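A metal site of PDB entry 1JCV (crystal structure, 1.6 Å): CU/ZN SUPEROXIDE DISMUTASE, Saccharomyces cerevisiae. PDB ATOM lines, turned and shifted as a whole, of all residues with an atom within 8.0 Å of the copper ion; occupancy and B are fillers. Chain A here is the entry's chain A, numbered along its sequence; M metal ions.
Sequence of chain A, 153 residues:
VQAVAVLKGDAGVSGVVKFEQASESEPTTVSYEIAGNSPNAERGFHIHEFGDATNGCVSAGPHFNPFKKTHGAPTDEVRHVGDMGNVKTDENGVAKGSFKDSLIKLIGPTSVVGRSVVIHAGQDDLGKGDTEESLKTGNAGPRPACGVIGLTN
O of Gly 141 is in hydrogen-bond range of ND1 of His 120 (2.9 Å).
O of Gly 61 is in hydrogen-bond range of ND1 of His 48 (2.7 Å).
O of Gly 44 sits at hydrogen-bond distance from N of His 120 (2.8 Å).
The backbone carbonyl oxygen of Pro 142 is in hydrogen-bond range of a ring nitrogen (ND1) of His 120 (3.1 Å).
ND1 of His 48 lies close to NH2 of Arg 143.
The backbone NH (N) of His 48 lies within hydrogen-bond range of the backbone carbonyl oxygen (O) of Ser 116 (2.8 Å).
NE2 of His 46 sits at hydrogen-bond distance from OD2 of Asp 124 (2.8 Å).
A ring nitrogen (ND1) of His 46 sits close to a ring nitrogen (NE2) of His 63 (3.2 Å).
His 63 touches the copper ion (NE2 to CU, 3.2 Å).
Within 4 Å of the copper ion: His 46, His 48, His 63 and His 120.
The copper ion is bound by NE2 of His 48.
The copper ion is bound by a ring nitrogen (NE2) of His 120 (2.1 Å).
ND1 of His 46 is bound to the copper ion, 2.1 Å away.
The copper ion has three donor atoms within binding distance.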
ATOM      1  N   GLY A  44      14.896 -29.067  31.955  1.00  0.00           N
ATOM      2  CA  GLY A  44      13.982 -27.944  31.795  1.00  0.00           C
ATOM      3  C   GLY A  44      13.100 -28.122  30.571  1.00  0.00           C
ATOM      4  O   GLY A  44      13.596 -28.459  29.494  1.00  0.00           O
ATOM      5  N   PHE A  45      11.833 -27.742  30.702  1.00  0.00           N
ATOM      6  CA  PHE A  45      10.849 -27.939  29.632  1.00  0.00           C
ATOM      7  C   PHE A  45       9.918 -26.716  29.636  1.00  0.00           C
ATOM      8  O   PHE A  45       9.260 -26.434  30.644  1.00  0.00           O
ATOM      9  CB  PHE A  45      10.093 -29.217  30.018  1.00  0.00           C
ATOM     10  CG  PHE A  45       9.125 -29.727  28.988  1.00  0.00           C
ATOM     11  CD1 PHE A  45       9.508 -29.909  27.663  1.00  0.00           C
ATOM     12  CD2 PHE A  45       7.846 -30.110  29.362  1.00  0.00           C
ATOM     13  CE1 PHE A  45       8.614 -30.467  26.734  1.00  0.00           C
ATOM     14  CE2 PHE A  45       6.943 -30.663  28.447  1.00  0.00           C
ATOM     15  CZ  PHE A  45       7.337 -30.841  27.129  1.00  0.00           C
ATOM     16  N   HIS A  46       9.885 -25.939  28.559  1.00  0.00           N
ATOM     17  CA  HIS A  46       9.036 -24.743  28.555  1.00  0.00           C
ATOM     18  C   HIS A  46       8.495 -24.365  27.195  1.00  0.00           C
ATOM     19  O   HIS A  46       8.997 -24.818  26.159  1.00  0.00           O
ATOM     20  CB  HIS A  46       9.790 -23.496  29.040  1.00  0.00           C
ATOM     21  CG  HIS A  46      10.848 -23.760  30.056  1.00  0.00           C
ATOM     22  ND1 HIS A  46      12.195 -23.769  29.745  1.00  0.00           N
ATOM     23  CD2 HIS A  46      10.760 -24.040  31.374  1.00  0.00           C
ATOM     24  CE1 HIS A  46      12.887 -24.062  30.827  1.00  0.00           C
ATOM     25  NE2 HIS A  46      12.040 -24.229  31.832  1.00  0.00           N
ATOM     26  N   ILE A  47       7.516 -23.469  27.208  1.00  0.00           N
ATOM     27  CA  ILE A  47       6.980 -22.912  25.993  1.00  0.00           C
ATOM     28  C   ILE A  47       7.675 -21.547  25.862  1.00  0.00           C
ATOM     29  O   ILE A  47       7.758 -20.790  26.824  1.00  0.00           O
ATOM     30  CB  ILE A  47       5.461 -22.758  26.078  1.00  0.00           C
ATOM     31  CG1 ILE A  47       4.848 -24.167  26.106  1.00  0.00           C
ATOM     32  CG2 ILE A  47       4.946 -21.967  24.875  1.00  0.00           C
ATOM     33  CD1 ILE A  47       3.377 -24.199  26.376  1.00  0.00           C
ATOM     34  N   HIS A  48       8.316 -21.343  24.708  1.00  0.00           N
ATOM     35  CA  HIS A  48       9.021 -20.104  24.414  1.00  0.00           C
ATOM     36  C   HIS A  48       8.131 -19.235  23.546  1.00  0.00           C
ATOM     37  O   HIS A  48       7.239 -19.751  22.849  1.00  0.00           O
ATOM     38  CB  HIS A  48      10.387 -20.388  23.780  1.00  0.00           C
ATOM     39  CG  HIS A  48      11.409 -20.885  24.746  1.00  0.00           C
ATOM     40  ND1 HIS A  48      12.636 -20.288  24.909  1.00  0.00           N
ATOM     41  CD2 HIS A  48      11.364 -21.904  25.641  1.00  0.00           C
ATOM     42  CE1 HIS A  48      13.313 -20.904  25.861  1.00  0.00           C
ATOM     43  NE2 HIS A  48      12.564 -21.900  26.328  1.00  0.00           N
ATOM     44  N   ALA A  60      13.466 -19.105  19.007  1.00  0.00           N
ATOM     45  CA  ALA A  60      12.230 -19.339  19.758  1.00  0.00           C
ATOM     46  C   ALA A  60      12.108 -18.198  20.791  1.00  0.00           C
ATOM     47  O   ALA A  60      11.035 -17.940  21.342  1.00  0.00           O
ATOM     48  CB  ALA A  60      12.297 -20.690  20.467  1.00  0.00           C
ATOM     49  N   GLY A  61      13.204 -17.513  21.052  1.00  0.00           N
ATOM     50  CA  GLY A  61      13.155 -16.422  21.985  1.00  0.00           C
ATOM     51  C   GLY A  61      13.141 -16.889  23.427  1.00  0.00           C
ATOM     52  O   GLY A  61      13.501 -18.029  23.711  1.00  0.00           O
ATOM     53  N   PRO A  62      12.661 -16.038  24.357  1.00  0.00           N
ATOM     54  CA  PRO A  62      12.576 -16.313  25.791  1.00  0.00           C
ATOM     55  C   PRO A  62      11.348 -17.125  26.193  1.00  0.00           C
ATOM     56  O   PRO A  62      10.536 -17.476  25.339  1.00  0.00           O
ATOM     57  CB  PRO A  62      12.515 -14.901  26.375  1.00  0.00           C
ATOM     58  CG  PRO A  62      11.637 -14.207  25.376  1.00  0.00           C
ATOM     59  CD  PRO A  62      12.206 -14.670  24.051  1.00  0.00           C
ATOM     60  N   HIS A  63      11.218 -17.442  27.474  1.00  0.00           N
ATOM     61  CA  HIS A  63      10.060 -18.177  27.957  1.00  0.00           C
ATOM     62  C   HIS A  63       8.837 -17.298  27.696  1.00  0.00           C
ATOM     63  O   HIS A  63       8.918 -16.071  27.838  1.00  0.00           O
ATOM     64  CB  HIS A  63      10.171 -18.459  29.459  1.00  0.00           C
ATOM     65  CG  HIS A  63      11.306 -19.361  29.804  1.00  0.00           C
ATOM     66  ND1 HIS A  63      11.506 -19.854  31.074  1.00  0.00           N
ATOM     67  CD2 HIS A  63      12.284 -19.876  29.035  1.00  0.00           C
ATOM     68  CE1 HIS A  63      12.578 -20.628  31.070  1.00  0.00           C
ATOM     69  NE2 HIS A  63      13.071 -20.662  29.843  1.00  0.00           N
ATOM     70  N   PHE A  64       7.740 -17.913  27.275  1.00  0.00           N
ATOM     71  CA  PHE A  64       6.514 -17.168  27.006  1.00  0.00           C
ATOM     72  C   PHE A  64       6.073 -16.592  28.359  1.00  0.00           C
ATOM     73  O   PHE A  64       5.832 -17.335  29.321  1.00  0.00           O
ATOM     74  CB  PHE A  64       5.468 -18.096  26.389  1.00  0.00           C
ATOM     75  CG  PHE A  64       4.169 -17.423  26.072  1.00  0.00           C
ATOM     76  CD1 PHE A  64       4.153 -16.161  25.505  1.00  0.00           C
ATOM     77  CD2 PHE A  64       2.954 -18.071  26.330  1.00  0.00           C
ATOM     78  CE1 PHE A  64       2.938 -15.541  25.211  1.00  0.00           C
ATOM     79  CE2 PHE A  64       1.735 -17.465  26.039  1.00  0.00           C
ATOM     80  CZ  PHE A  64       1.719 -16.193  25.482  1.00  0.00           C
ATOM     81  N   HIS A  71      10.426 -16.301  36.486  1.00  0.00           N
ATOM     82  CA  HIS A  71      10.452 -17.734  36.202  1.00  0.00           C
ATOM     83  C   HIS A  71      10.194 -18.516  37.489  1.00  0.00           C
ATOM     84  O   HIS A  71      10.770 -18.198  38.534  1.00  0.00           O
ATOM     85  CB  HIS A  71      11.837 -18.088  35.647  1.00  0.00           C
ATOM     86  CG  HIS A  71      12.014 -19.546  35.414  1.00  0.00           C
ATOM     87  ND1 HIS A  71      11.525 -20.181  34.299  1.00  0.00           N
ATOM     88  CD2 HIS A  71      12.564 -20.508  36.192  1.00  0.00           C
ATOM     89  CE1 HIS A  71      11.744 -21.485  34.411  1.00  0.00           C
ATOM     90  NE2 HIS A  71      12.365 -21.698  35.550  1.00  0.00           N
ATOM     91  N   GLY A  82       4.695 -20.037  30.163  1.00  0.00           N
ATOM     92  CA  GLY A  82       5.358 -21.189  29.553  1.00  0.00           C
ATOM     93  C   GLY A  82       6.146 -22.153  30.426  1.00  0.00           C
ATOM     94  O   GLY A  82       6.681 -23.135  29.914  1.00  0.00           O
ATOM     95  N   ASP A  83       6.219 -21.904  31.726  1.00  0.00           N
ATOM     96  CA  ASP A  83       6.979 -22.752  32.629  1.00  0.00           C
ATOM     97  C   ASP A  83       6.368 -24.120  32.890  1.00  0.00           C
ATOM     98  O   ASP A  83       5.326 -24.245  33.549  1.00  0.00           O
ATOM     99  CB  ASP A  83       7.242 -22.023  33.952  1.00  0.00           C
ATOM    100  CG  ASP A  83       8.219 -20.858  33.807  1.00  0.00           C
ATOM    101  OD1 ASP A  83       8.945 -20.768  32.782  1.00  0.00           O
ATOM    102  OD2 ASP A  83       8.297 -20.003  34.706  1.00  0.00           O
ATOM    103  N   MET A  84       7.000 -25.151  32.343  1.00  0.00           N
ATOM    104  CA  MET A  84       6.563 -26.535  32.532  1.00  0.00           C
ATOM    105  C   MET A  84       7.549 -27.328  33.418  1.00  0.00           C
ATOM    106  O   MET A  84       7.502 -28.558  33.465  1.00  0.00           O
ATOM    107  CB  MET A  84       6.333 -27.210  31.185  1.00  0.00           C
ATOM    108  CG  MET A  84       5.337 -26.449  30.324  1.00  0.00           C
ATOM    109  SD  MET A  84       4.832 -27.359  28.855  1.00  0.00           S
ATOM    110  CE  MET A  84       6.304 -27.223  27.819  1.00  0.00           C
ATOM    111  N   GLY A  85       8.425 -26.620  34.129  1.00  0.00           N
ATOM    112  CA  GLY A  85       9.363 -27.261  35.042  1.00  0.00           C
ATOM    113  C   GLY A  85      10.374 -28.209  34.412  1.00  0.00           C
ATOM    114  O   GLY A  85      10.986 -27.883  33.395  1.00  0.00           O
ATOM    115  N   SER A 116       6.615 -21.968  20.584  1.00  0.00           N
ATOM    116  CA  SER A 116       7.521 -23.115  20.524  1.00  0.00           C
ATOM    117  C   SER A 116       7.658 -23.836  21.840  1.00  0.00           C
ATOM    118  O   SER A 116       7.452 -23.246  22.907  1.00  0.00           O
ATOM    119  CB  SER A 116       8.941 -22.681  20.120  1.00  0.00           C
ATOM    120  OG  SER A 116       9.070 -22.222  18.786  1.00  0.00           O
ATOM    121  N   VAL A 117       8.023 -25.117  21.763  1.00  0.00           N
ATOM    122  CA  VAL A 117       8.296 -25.900  22.967  1.00  0.00           C
ATOM    123  C   VAL A 117       9.801 -26.144  22.909  1.00  0.00           C
ATOM    124  O   VAL A 117      10.326 -26.445  21.832  1.00  0.00           O
ATOM    125  CB  VAL A 117       7.620 -27.278  22.964  1.00  0.00           C
ATOM    126  CG1 VAL A 117       8.102 -28.073  24.168  1.00  0.00           C
ATOM    127  CG2 VAL A 117       6.109 -27.147  23.004  1.00  0.00           C
ATOM    128  N   VAL A 118      10.495 -25.971  24.030  1.00  0.00           N
ATOM    129  CA  VAL A 118      11.938 -26.206  24.079  1.00  0.00           C
ATOM    130  C   VAL A 118      12.254 -27.173  25.227  1.00  0.00           C
ATOM    131  O   VAL A 118      11.709 -27.032  26.334  1.00  0.00           O
ATOM    132  CB  VAL A 118      12.726 -24.888  24.297  1.00  0.00           C
ATOM    133  CG1 VAL A 118      14.186 -25.179  24.607  1.00  0.00           C
ATOM    134  CG2 VAL A 118      12.633 -23.983  23.081  1.00  0.00           C
ATOM    135  N   ILE A 119      13.073 -28.187  24.922  1.00  0.00           N
ATOM    136  CA  ILE A 119      13.539 -29.158  25.920  1.00  0.00           C
ATOM    137  C   ILE A 119      15.013 -28.783  26.103  1.00  0.00           C
ATOM    138  O   ILE A 119      15.751 -28.617  25.127  1.00  0.00           O
ATOM    139  CB  ILE A 119      13.372 -30.660  25.493  1.00  0.00           C
ATOM    140  CG1 ILE A 119      13.968 -31.580  26.562  1.00  0.00           C
ATOM    141  CG2 ILE A 119      14.024 -30.943  24.137  1.00  0.00           C
ATOM    142  CD1 ILE A 119      13.266 -31.529  27.895  1.00  0.00           C
ATOM    143  N   HIS A 120      15.405 -28.599  27.363  1.00  0.00           N
ATOM    144  CA  HIS A 120      16.754 -28.176  27.706  1.00  0.00           C
ATOM    145  C   HIS A 120      17.733 -29.284  28.034  1.00  0.00           C
ATOM    146  O   HIS A 120      17.330 -30.413  28.336  1.00  0.00           O
ATOM    147  CB  HIS A 120      16.706 -27.177  28.862  1.00  0.00           C
ATOM    148  CG  HIS A 120      16.135 -25.851  28.471  1.00  0.00           C
ATOM    149  ND1 HIS A 120      16.921 -24.800  28.055  1.00  0.00           N
ATOM    150  CD2 HIS A 120      14.850 -25.432  28.375  1.00  0.00           C
ATOM    151  CE1 HIS A 120      16.145 -23.793  27.708  1.00  0.00           C
ATOM    152  NE2 HIS A 120      14.884 -24.137  27.896  1.00  0.00           N
ATOM    153  N   ASP A 124      16.197 -27.335  35.469  1.00  0.00           N
ATOM    154  CA  ASP A 124      15.593 -26.041  35.728  1.00  0.00           C
ATOM    155  C   ASP A 124      15.589 -25.899  37.247  1.00  0.00           C
ATOM    156  O   ASP A 124      15.060 -26.768  37.920  1.00  0.00           O
ATOM    157  CB  ASP A 124      14.154 -26.082  35.180  1.00  0.00           C
ATOM    158  CG  ASP A 124      13.404 -24.759  35.310  1.00  0.00           C
ATOM    159  OD1 ASP A 124      13.726 -23.942  36.197  1.00  0.00           O
ATOM    160  OD2 ASP A 124      12.456 -24.560  34.532  1.00  0.00           O
ATOM    161  N   LYS A 136      15.003 -15.802  35.348  1.00  0.00           N
ATOM    162  CA  LYS A 136      14.739 -15.628  33.922  1.00  0.00           C
ATOM    163  C   LYS A 136      14.572 -16.939  33.153  1.00  0.00           C
ATOM    164  O   LYS A 136      13.581 -17.129  32.436  1.00  0.00           O
ATOM    165  CB  LYS A 136      15.879 -14.858  33.243  1.00  0.00           C
ATOM    166  CG  LYS A 136      16.115 -13.471  33.753  1.00  0.00           C
ATOM    167  CD  LYS A 136      17.133 -12.802  32.853  1.00  0.00           C
ATOM    168  CE  LYS A 136      17.647 -11.493  33.424  1.00  0.00           C
ATOM    169  NZ  LYS A 136      18.409 -10.750  32.350  1.00  0.00           N
ATOM    170  N   THR A 137      15.545 -17.834  33.322  1.00  0.00           N
ATOM    171  CA  THR A 137      15.562 -19.099  32.604  1.00  0.00           C
ATOM    172  C   THR A 137      15.607 -20.315  33.522  1.00  0.00           C
ATOM    173  O   THR A 137      15.502 -21.431  33.048  1.00  0.00           O
ATOM    174  CB  THR A 137      16.838 -19.187  31.746  1.00  0.00           C
ATOM    175  OG1 THR A 137      17.987 -19.178  32.599  1.00  0.00           O
ATOM    176  CG2 THR A 137      16.942 -18.019  30.808  1.00  0.00           C
ATOM    177  N   ALA A 140      18.404 -23.390  33.110  1.00  0.00           N
ATOM    178  CA  ALA A 140      18.201 -24.665  32.428  1.00  0.00           C
ATOM    179  C   ALA A 140      19.215 -24.962  31.326  1.00  0.00           C
ATOM    180  O   ALA A 140      19.268 -26.087  30.817  1.00  0.00           O
ATOM    181  CB  ALA A 140      16.781 -24.768  31.906  1.00  0.00           C
ATOM    182  N   GLY A 141      20.012 -23.961  30.969  1.00  0.00           N
ATOM    183  CA  GLY A 141      21.046 -24.177  29.976  1.00  0.00           C
ATOM    184  C   GLY A 141      20.644 -24.277  28.516  1.00  0.00           C
ATOM    185  O   GLY A 141      19.598 -23.760  28.110  1.00  0.00           O
ATOM    186  N   PRO A 142      21.451 -24.977  27.692  1.00  0.00           N
ATOM    187  CA  PRO A 142      21.237 -25.192  26.252  1.00  0.00           C
ATOM    188  C   PRO A 142      19.876 -25.746  25.850  1.00  0.00           C
ATOM    189  O   PRO A 142      19.171 -26.351  26.659  1.00  0.00           O
ATOM    190  CB  PRO A 142      22.376 -26.129  25.863  1.00  0.00           C
ATOM    191  CG  PRO A 142      23.463 -25.793  26.864  1.00  0.00           C
ATOM    192  CD  PRO A 142      22.669 -25.667  28.155  1.00  0.00           C
ATOM    193  N   ARG A 143      19.545 -25.572  24.565  1.00  0.00           N
ATOM    194  CA  ARG A 143      18.291 -26.000  23.986  1.00  0.00           C
ATOM    195  C   ARG A 143      18.585 -27.014  22.891  1.00  0.00           C
ATOM    196  O   ARG A 143      18.601 -26.667  21.704  1.00  0.00           O
ATOM    197  CB  ARG A 143      17.578 -24.802  23.340  1.00  0.00           C
ATOM    198  CG  ARG A 143      17.464 -23.564  24.209  1.00  0.00           C
ATOM    199  CD  ARG A 143      16.866 -22.392  23.447  1.00  0.00           C
ATOM    200  NE  ARG A 143      16.707 -21.243  24.323  1.00  0.00           N
ATOM    201  CZ  ARG A 143      16.025 -20.141  24.016  1.00  0.00           C
ATOM    202  NH1 ARG A 143      15.433 -20.018  22.825  1.00  0.00           N
ATOM    203  NH2 ARG A 143      15.906 -19.180  24.922  1.00  0.00           N
ATOM    204  N   ALA A 145      16.772 -29.379  21.604  1.00  0.00           N
ATOM    205  CA  ALA A 145      15.689 -29.598  20.654  1.00  0.00           C
ATOM    206  C   ALA A 145      14.515 -28.666  20.907  1.00  0.00           C
ATOM    207  O   ALA A 145      14.304 -28.202  22.040  1.00  0.00           O
ATOM    208  CB  ALA A 145      15.232 -31.055  20.680  1.00  0.00           C
HETATM  209 CU    CU M   1      13.021 -23.159  27.895  1.00  0.00          CU
HETATM  210 ZN    ZN M   2      10.349 -19.465  32.706  1.00  0.00          ZN
